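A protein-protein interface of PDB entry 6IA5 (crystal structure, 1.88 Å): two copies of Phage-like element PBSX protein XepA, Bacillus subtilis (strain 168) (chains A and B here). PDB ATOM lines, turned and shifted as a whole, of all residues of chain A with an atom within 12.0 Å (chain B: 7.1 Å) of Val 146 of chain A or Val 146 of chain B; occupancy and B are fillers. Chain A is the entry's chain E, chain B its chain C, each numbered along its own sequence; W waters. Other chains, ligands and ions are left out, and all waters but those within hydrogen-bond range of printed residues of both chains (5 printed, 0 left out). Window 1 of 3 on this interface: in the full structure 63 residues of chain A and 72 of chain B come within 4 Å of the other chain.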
ATOM      1  N   ASN A  35       4.142  10.364 -11.260  1.00  0.00           N
ATOM      2  CA  ASN A  35       2.711  10.257 -11.448  1.00  0.00           C
ATOM      3  C   ASN A  35       2.162   9.396 -10.319  1.00  0.00           C
ATOM      4  O   ASN A  35       2.846   8.485  -9.861  1.00  0.00           O
ATOM      5  CB  ASN A  35       2.377   9.655 -12.816  1.00  0.00           C
ATOM      6  CG  ASN A  35       0.886   9.628 -13.052  1.00  0.00           C
ATOM      7  OD1 ASN A  35       0.274   8.573 -12.930  1.00  0.00           O
ATOM      8  ND2 ASN A  35       0.279  10.771 -13.313  1.00  0.00           N
ATOM      9  N   GLY A 142      -6.587  10.496 -15.212  1.00  0.00           N
ATOM     10  CA  GLY A 142      -6.257  11.559 -16.154  1.00  0.00           C
ATOM     11  C   GLY A 142      -5.580  11.058 -17.433  1.00  0.00           C
ATOM     12  O   GLY A 142      -5.359   9.844 -17.631  1.00  0.00           O
ATOM     13  N   GLU A 143      -5.273  12.019 -18.312  1.00  0.00           N
ATOM     14  CA  GLU A 143      -4.694  11.711 -19.602  1.00  0.00           C
ATOM     15  C   GLU A 143      -4.066  12.976 -20.154  1.00  0.00           C
ATOM     16  O   GLU A 143      -4.736  13.993 -20.274  1.00  0.00           O
ATOM     17  CB  GLU A 143      -5.743  11.156 -20.571  1.00  0.00           C
ATOM     18  CG  GLU A 143      -5.121  10.664 -21.877  1.00  0.00           C
ATOM     19  CD  GLU A 143      -6.086   9.881 -22.776  1.00  0.00           C
ATOM     20  OE1 GLU A 143      -6.903  10.495 -23.437  1.00  0.00           O
ATOM     21  OE2 GLU A 143      -6.034   8.643 -22.792  1.00  0.00           O
ATOM     22  N   MET A 144      -2.782  12.890 -20.517  1.00  0.00           N
ATOM     23  CA  MET A 144      -2.011  14.032 -20.985  1.00  0.00           C
ATOM     24  C   MET A 144      -1.895  13.973 -22.512  1.00  0.00           C
ATOM     25  O   MET A 144      -1.607  12.907 -23.090  1.00  0.00           O
ATOM     26  CB  MET A 144      -0.615  13.934 -20.355  1.00  0.00           C
ATOM     27  CG  MET A 144       0.400  15.037 -20.701  1.00  0.00           C
ATOM     28  SD  MET A 144       2.013  14.443 -20.042  1.00  0.00           S
ATOM     29  CE  MET A 144       1.561  14.106 -18.336  1.00  0.00           C
ATOM     30  N   ASP A 145      -2.092  15.136 -23.154  1.00  0.00           N
ATOM     31  CA  ASP A 145      -1.854  15.296 -24.585  1.00  0.00           C
ATOM     32  C   ASP A 145      -0.349  15.404 -24.809  1.00  0.00           C
ATOM     33  O   ASP A 145       0.334  16.149 -24.092  1.00  0.00           O
ATOM     34  CB  ASP A 145      -2.622  16.492 -25.173  1.00  0.00           C
ATOM     35  CG  ASP A 145      -4.126  16.253 -25.033  1.00  0.00           C
ATOM     36  OD1 ASP A 145      -4.638  15.411 -25.731  1.00  0.00           O
ATOM     37  OD2 ASP A 145      -4.752  16.828 -24.134  1.00  0.00           O
ATOM     38  N   VAL A 146       0.158  14.640 -25.789  1.00  0.00           N
ATOM     39  CA  VAL A 146       1.566  14.680 -26.144  1.00  0.00           C
ATOM     40  C   VAL A 146       1.716  14.862 -27.653  1.00  0.00           C
ATOM     41  O   VAL A 146       0.825  14.520 -28.428  1.00  0.00           O
ATOM     42  CB  VAL A 146       2.319  13.435 -25.637  1.00  0.00           C
ATOM     43  CG1 VAL A 146       2.188  13.274 -24.111  1.00  0.00           C
ATOM     44  CG2 VAL A 146       1.898  12.150 -26.350  1.00  0.00           C
ATOM     45  N   ARG A 147       2.853  15.444 -28.055  1.00  0.00           N
ATOM     46  CA  ARG A 147       3.240  15.609 -29.441  1.00  0.00           C
ATOM     47  C   ARG A 147       4.493  14.774 -29.651  1.00  0.00           C
ATOM     48  O   ARG A 147       5.534  15.038 -29.024  1.00  0.00           O
ATOM     49  CB  ARG A 147       3.501  17.081 -29.787  1.00  0.00           C
ATOM     50  CG  ARG A 147       3.979  17.337 -31.219  1.00  0.00           C
ATOM     51  CD  ARG A 147       2.850  17.233 -32.237  1.00  0.00           C
ATOM     52  NE  ARG A 147       1.795  18.200 -31.941  1.00  0.00           N
ATOM     53  CZ  ARG A 147       1.621  19.388 -32.531  1.00  0.00           C
ATOM     54  NH1 ARG A 147       2.346  19.723 -33.589  1.00  0.00           N
ATOM     55  NH2 ARG A 147       0.720  20.236 -32.059  1.00  0.00           N
ATOM     56  N   VAL A 148       4.383  13.800 -30.566  1.00  0.00           N
ATOM     57  CA  VAL A 148       5.510  12.927 -30.869  1.00  0.00           C
ATOM     58  C   VAL A 148       6.503  13.658 -31.760  1.00  0.00           C
ATOM     59  O   VAL A 148       6.107  14.244 -32.760  1.00  0.00           O
ATOM     60  CB  VAL A 148       5.062  11.586 -31.480  1.00  0.00           C
ATOM     61  CG1 VAL A 148       6.262  10.771 -31.949  1.00  0.00           C
ATOM     62  CG2 VAL A 148       4.306  10.789 -30.426  1.00  0.00           C
ATOM     63  N   ASN A 149       7.784  13.633 -31.361  1.00  0.00           N
ATOM     64  CA  ASN A 149       8.830  14.311 -32.099  1.00  0.00           C
ATOM     65  C   ASN A 149       8.909  13.746 -33.518  1.00  0.00           C
ATOM     66  O   ASN A 149       8.998  12.533 -33.691  1.00  0.00           O
ATOM     67  CB  ASN A 149      10.173  14.198 -31.367  1.00  0.00           C
ATOM     68  CG  ASN A 149      11.254  15.008 -32.062  1.00  0.00           C
ATOM     69  OD1 ASN A 149      11.605  14.707 -33.195  1.00  0.00           O
ATOM     70  ND2 ASN A 149      11.757  16.053 -31.429  1.00  0.00           N
ATOM     71  N   GLU A 150       8.947  14.644 -34.514  1.00  0.00           N
ATOM     72  CA  GLU A 150       8.880  14.283 -35.925  1.00  0.00           C
ATOM     73  C   GLU A 150      10.258  13.955 -36.508  1.00  0.00           C
ATOM     74  O   GLU A 150      10.350  13.468 -37.623  1.00  0.00           O
ATOM     75  CB  GLU A 150       8.173  15.390 -36.699  1.00  0.00           C
ATOM     76  CG  GLU A 150       6.703  15.460 -36.339  1.00  0.00           C
ATOM     77  CD  GLU A 150       6.195  16.792 -35.807  1.00  0.00           C
ATOM     78  OE1 GLU A 150       7.023  17.620 -35.372  1.00  0.00           O
ATOM     79  OE2 GLU A 150       4.961  16.976 -35.773  1.00  0.00           O
ATOM     80  N   LYS A 151      11.330  14.169 -35.740  1.00  0.00           N
ATOM     81  CA  LYS A 151      12.690  13.969 -36.225  1.00  0.00           C
ATOM     82  C   LYS A 151      12.889  12.529 -36.687  1.00  0.00           C
ATOM     83  O   LYS A 151      13.380  12.304 -37.788  1.00  0.00           O
ATOM     84  CB  LYS A 151      13.753  14.367 -35.187  1.00  0.00           C
ATOM     85  CG  LYS A 151      15.072  13.600 -35.262  1.00  0.00           C
ATOM     86  CD  LYS A 151      16.278  14.341 -34.725  1.00  0.00           C
ATOM     87  CE  LYS A 151      17.563  13.614 -35.050  1.00  0.00           C
ATOM     88  NZ  LYS A 151      18.723  14.273 -34.413  1.00  0.00           N
ATOM     89  N   THR A 152      12.554  11.561 -35.828  1.00  0.00           N
ATOM     90  CA  THR A 152      12.835  10.176 -36.167  1.00  0.00           C
ATOM     91  C   THR A 152      11.522   9.457 -36.475  1.00  0.00           C
ATOM     92  O   THR A 152      10.559   9.543 -35.719  1.00  0.00           O
ATOM     93  CB  THR A 152      13.736   9.494 -35.128  1.00  0.00           C
ATOM     94  OG1 THR A 152      13.671  10.263 -33.924  1.00  0.00           O
ATOM     95  CG2 THR A 152      15.172   9.354 -35.590  1.00  0.00           C
ATOM     96  N   PRO A 153      11.424   8.770 -37.631  1.00  0.00           N
ATOM     97  CA  PRO A 153      10.275   7.904 -37.904  1.00  0.00           C
ATOM     98  C   PRO A 153      10.166   6.894 -36.764  1.00  0.00           C
ATOM     99  O   PRO A 153      11.181   6.496 -36.210  1.00  0.00           O
ATOM    100  CB  PRO A 153      10.667   7.197 -39.214  1.00  0.00           C
ATOM    101  CG  PRO A 153      11.651   8.146 -39.879  1.00  0.00           C
ATOM    102  CD  PRO A 153      12.399   8.801 -38.732  1.00  0.00           C
ATOM    103  N   LEU A 154       8.947   6.499 -36.407  1.00  0.00           N
ATOM    104  CA  LEU A 154       8.731   5.376 -35.506  1.00  0.00           C
ATOM    105  C   LEU A 154       8.920   4.057 -36.252  1.00  0.00           C
ATOM    106  O   LEU A 154       8.412   3.893 -37.360  1.00  0.00           O
ATOM    107  CB  LEU A 154       7.301   5.462 -34.965  1.00  0.00           C
ATOM    108  CG  LEU A 154       6.941   6.775 -34.279  1.00  0.00           C
ATOM    109  CD1 LEU A 154       5.509   6.735 -33.754  1.00  0.00           C
ATOM    110  CD2 LEU A 154       7.921   7.055 -33.150  1.00  0.00           C
ATOM    111  N   GLY B 142      -2.919  22.087 -22.373  1.00  0.00           N
ATOM    112  CA  GLY B 142      -1.525  21.959 -22.772  1.00  0.00           C
ATOM    113  C   GLY B 142      -1.240  20.701 -23.601  1.00  0.00           C
ATOM    114  O   GLY B 142      -2.130  19.896 -23.911  1.00  0.00           O
ATOM    115  N   GLU B 143       0.033  20.571 -23.970  1.00  0.00           N
ATOM    116  CA  GLU B 143       0.529  19.475 -24.771  1.00  0.00           C
ATOM    117  C   GLU B 143       2.044  19.413 -24.571  1.00  0.00           C
ATOM    118  O   GLU B 143       2.740  20.411 -24.773  1.00  0.00           O
ATOM    119  CB  GLU B 143       0.179  19.731 -26.240  1.00  0.00           C
ATOM    120  CG  GLU B 143       0.624  18.593 -27.155  1.00  0.00           C
ATOM    121  CD  GLU B 143       0.160  18.677 -28.602  1.00  0.00           C
ATOM    122  OE1 GLU B 143       0.603  19.553 -29.357  1.00  0.00           O
ATOM    123  OE2 GLU B 143      -0.642  17.844 -28.964  1.00  0.00           O
ATOM    124  N   MET B 144       2.543  18.225 -24.215  1.00  0.00           N
ATOM    125  CA  MET B 144       3.964  18.011 -23.961  1.00  0.00           C
ATOM    126  C   MET B 144       4.618  17.331 -25.173  1.00  0.00           C
ATOM    127  O   MET B 144       4.066  16.381 -25.739  1.00  0.00           O
ATOM    128  CB  MET B 144       4.121  17.097 -22.735  1.00  0.00           C
ATOM    129  CG  MET B 144       5.576  16.861 -22.268  1.00  0.00           C
ATOM    130  SD  MET B 144       6.373  18.411 -21.799  1.00  0.00           S
ATOM    131  CE  MET B 144       8.123  18.065 -21.980  1.00  0.00           C
ATOM    132  N   ASP B 145       5.805  17.820 -25.571  1.00  0.00           N
ATOM    133  CA  ASP B 145       6.628  17.164 -26.578  1.00  0.00           C
ATOM    134  C   ASP B 145       7.287  15.929 -25.957  1.00  0.00           C
ATOM    135  O   ASP B 145       7.846  16.007 -24.854  1.00  0.00           O
ATOM    136  CB  ASP B 145       7.639  18.097 -27.244  1.00  0.00           C
ATOM    137  CG  ASP B 145       6.905  19.246 -27.925  1.00  0.00           C
ATOM    138  OD1 ASP B 145       6.288  18.999 -28.962  1.00  0.00           O
ATOM    139  OD2 ASP B 145       6.863  20.386 -27.363  1.00  0.00           O
ATOM    140  N   VAL B 146       7.191  14.792 -26.662  1.00  0.00           N
ATOM    141  CA  VAL B 146       7.810  13.558 -26.203  1.00  0.00           C
ATOM    142  C   VAL B 146       8.653  12.958 -27.320  1.00  0.00           C
ATOM    143  O   VAL B 146       8.410  13.202 -28.511  1.00  0.00           O
ATOM    144  CB  VAL B 146       6.761  12.553 -25.667  1.00  0.00           C
ATOM    145  CG1 VAL B 146       5.926  13.167 -24.544  1.00  0.00           C
ATOM    146  CG2 VAL B 146       5.833  12.048 -26.789  1.00  0.00           C
ATOM    147  N   ARG B 147       9.674  12.199 -26.895  1.00  0.00           N
ATOM    148  CA  ARG B 147      10.516  11.429 -27.792  1.00  0.00           C
ATOM    149  C   ARG B 147      10.323   9.958 -27.445  1.00  0.00           C
ATOM    150  O   ARG B 147      10.628   9.540 -26.322  1.00  0.00           O
ATOM    151  CB  ARG B 147      11.992  11.808 -27.613  1.00  0.00           C
ATOM    152  CG  ARG B 147      12.940  11.074 -28.558  1.00  0.00           C
ATOM    153  CD  ARG B 147      12.906  11.657 -29.959  1.00  0.00           C
ATOM    154  NE  ARG B 147      13.282  13.073 -29.923  1.00  0.00           N
ATOM    155  CZ  ARG B 147      14.463  13.582 -30.292  1.00  0.00           C
ATOM    156  NH1 ARG B 147      15.356  12.819 -30.884  1.00  0.00           N
ATOM    157  NH2 ARG B 147      14.746  14.858 -30.085  1.00  0.00           N
ATOM    158  N   VAL B 148       9.811   9.197 -28.400  1.00  0.00           N
ATOM    159  CA  VAL B 148       9.433   7.801 -28.177  1.00  0.00           C
ATOM    160  C   VAL B 148      10.689   6.930 -28.206  1.00  0.00           C
ATOM    161  O   VAL B 148      11.482   7.041 -29.130  1.00  0.00           O
ATOM    162  CB  VAL B 148       8.404   7.319 -29.225  1.00  0.00           C
ATOM    163  CG1 VAL B 148       8.152   5.825 -29.107  1.00  0.00           C
ATOM    164  CG2 VAL B 148       7.105   8.081 -29.084  1.00  0.00           C
HETATM  165  O   HOH W   1      -4.591  19.548 -24.033  1.00  0.00           O
HETATM  166  O   HOH W   2      17.969  14.055 -31.398  1.00  0.00           O
HETATM  167  O   HOH W   3       7.562  17.047 -30.332  1.00  0.00           O
HETATM  168  O   HOH W   4      14.897   9.602 -31.139  1.00  0.00           O
HETATM  169  O   HOH W   5      -2.956  17.638 -21.903  1.00  0.00           O
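The side-chain carboxylate (OE1) of Glu 143 of chain B lies within salt-bridge range of the guanidinium group (NH2) of Arg 147 of chain A, 2.8 Å away.
The backbone NH (N) of Met 144 of chain B sits at hydrogen-bond distance from the backbone carbonyl oxygen (O) of Asp 145 of chain A.
The backbone NH (N) of Arg 147 of chain A lies within hydrogen-bond range of the backbone carbonyl oxygen (O) of Met 144 of chain B.
N of Val 146 of chain B is in hydrogen-bond range of O of Arg 147 of chain A, at 2.9 Å.
The backbone NH (N) of Asn 149 of chain A is in hydrogen-bond range of the backbone carbonyl oxygen (O) of Val 146 of chain B (2.9 Å).
The guanidinium group (NH2) of Arg 147 of chain B sits close to the side-chain amide nitrogen (ND2) of Asn 149 of chain A.
The side-chain amide oxygen of Asn 149 of chain A sits at hydrogen-bond distance from the backbone NH of Lys 151 of chain A (2.6 Å).
Hydrophobic or aromatic side chains of chain A that line the printed part of chain B: Val 146 and Leu 154.
Along chain A the printed residues that touch a printed residue of chain B span positions 145 to 154.
Of the 7 printed residues of chain B, 7 touch a printed residue of chain A.
Printed residues of chain B that touch a printed residue of chain A: Gly 142, Glu 143, Met 144, Asp 145, Val 146, Arg 147 and Val 148.
Hydrophobic or aromatic side chains of chain B within 4 Å of the printed part of chain A: Val 146 and Val 148.
Among the printed residues, 14 pairs touch across the chains.
Among the printed residues, Asp or Glu carboxylates within 4 Å of a Lys or Arg side-chain nitrogen of the other chain: Arg 147 of chain A with Glu 143 of chain B (2.8 Å).
Asp 145 of chain A touches Gly 142 of chain B (CB to O, 3.7 Å).
O of Asp 145 of chain A touches CA of Glu 143 of chain B (3.4 Å).
O of Val 146 of chain A touches OE2 of Glu 143 of chain B, at 3.7 Å.
Val 146 of chain A touches Met 144 of chain B.
Val 146 of chain A touches Val 146 of chain B.
O of Arg 147 of chain A touches CA of Asp 145 of chain B (3.4 Å).
CA of Val 148 of chain A touches O of Val 146 of chain B, 3.7 Å away.
Leu 154 of chain A touches Val 148 of chain B (CD2 to CB, 3.96 Å).
Asp 145 of chain A touches Glu 143 of chain B, but with the chains exchanged Glu 143 of chain A does not touch Asp 145 of chain B (12.3 Å).
Val 146 of chain B touches its own counterpart, Val 146 of chain A.
Arg 147 of chain A touches Met 144 of chain B, but with the chains exchanged Met 144 of chain A does not touch Arg 147 of chain B (10.5 Å).
Val 148 of chain A touches Val 146 of chain B, but with the chains exchanged Val 146 of chain A does not touch Val 148 of chain B (7.2 Å).
Of the 14 pairs that touch across the chains among the printed residues, 1 has its exchanged pair printed and touching as well.
Water W1 lies within hydrogen-bond range of O of Gly 142 of chain B (2.5 Å) and OD2 of Asp 145 of chain A (2.7 Å).
Water W3 lies within hydrogen-bond range of OD1 of Asp 145 of chain B (2.7 Å) and O of Arg 147 of chain A (3.1 Å).
Water W5 lies within hydrogen-bond range of the backbone NH (N) of Asp 145 of chain A (2.9 Å) and the backbone carbonyl oxygen (O) of Gly 142 of chain B (3.1 Å).
Water W2 lies within hydrogen-bond range of NH1 of Arg 147 of chain B (2.9 Å) and NZ of Lys 151 of chain A (3.1 Å).
Water W4 lies within hydrogen-bond range of the side-chain hydroxyl of Thr 152 of chain A and the guanidinium group of Arg 147 of chain B.
Met 144 of chain A touches none of the printed residues of chain B.
Of the printed residues of chain B, Val 146 of chain A touches Glu 143, Met 144 and Val 146.
Of the printed residues of chain B, Val 148 of chain A touches Val 146.
Printed residues of chain B within 4 Å of Asn 149 of chain A: Val 146 and Arg 147.
Lys 151 of chain A touches none of the printed residues of chain B.
Of the printed residues of chain A, Met 144 of chain B touches Asp 145 (3.0 Å), Val 146 (3.1 Å) and Arg 147 (2.8 Å).
Of chain A, only Arg 147 (3.4 Å) comes within 4 Å of Asp 145 of chain B.
Arg 147 of chain B touches one residue of chain A.
Of the printed residues of chain A, Val 148 of chain B touches Leu 154 (3.96 Å).
The nearest printed residue of chain B that does not touch Val 146 of chain A is Asp 145 of chain B (5.3 Å).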
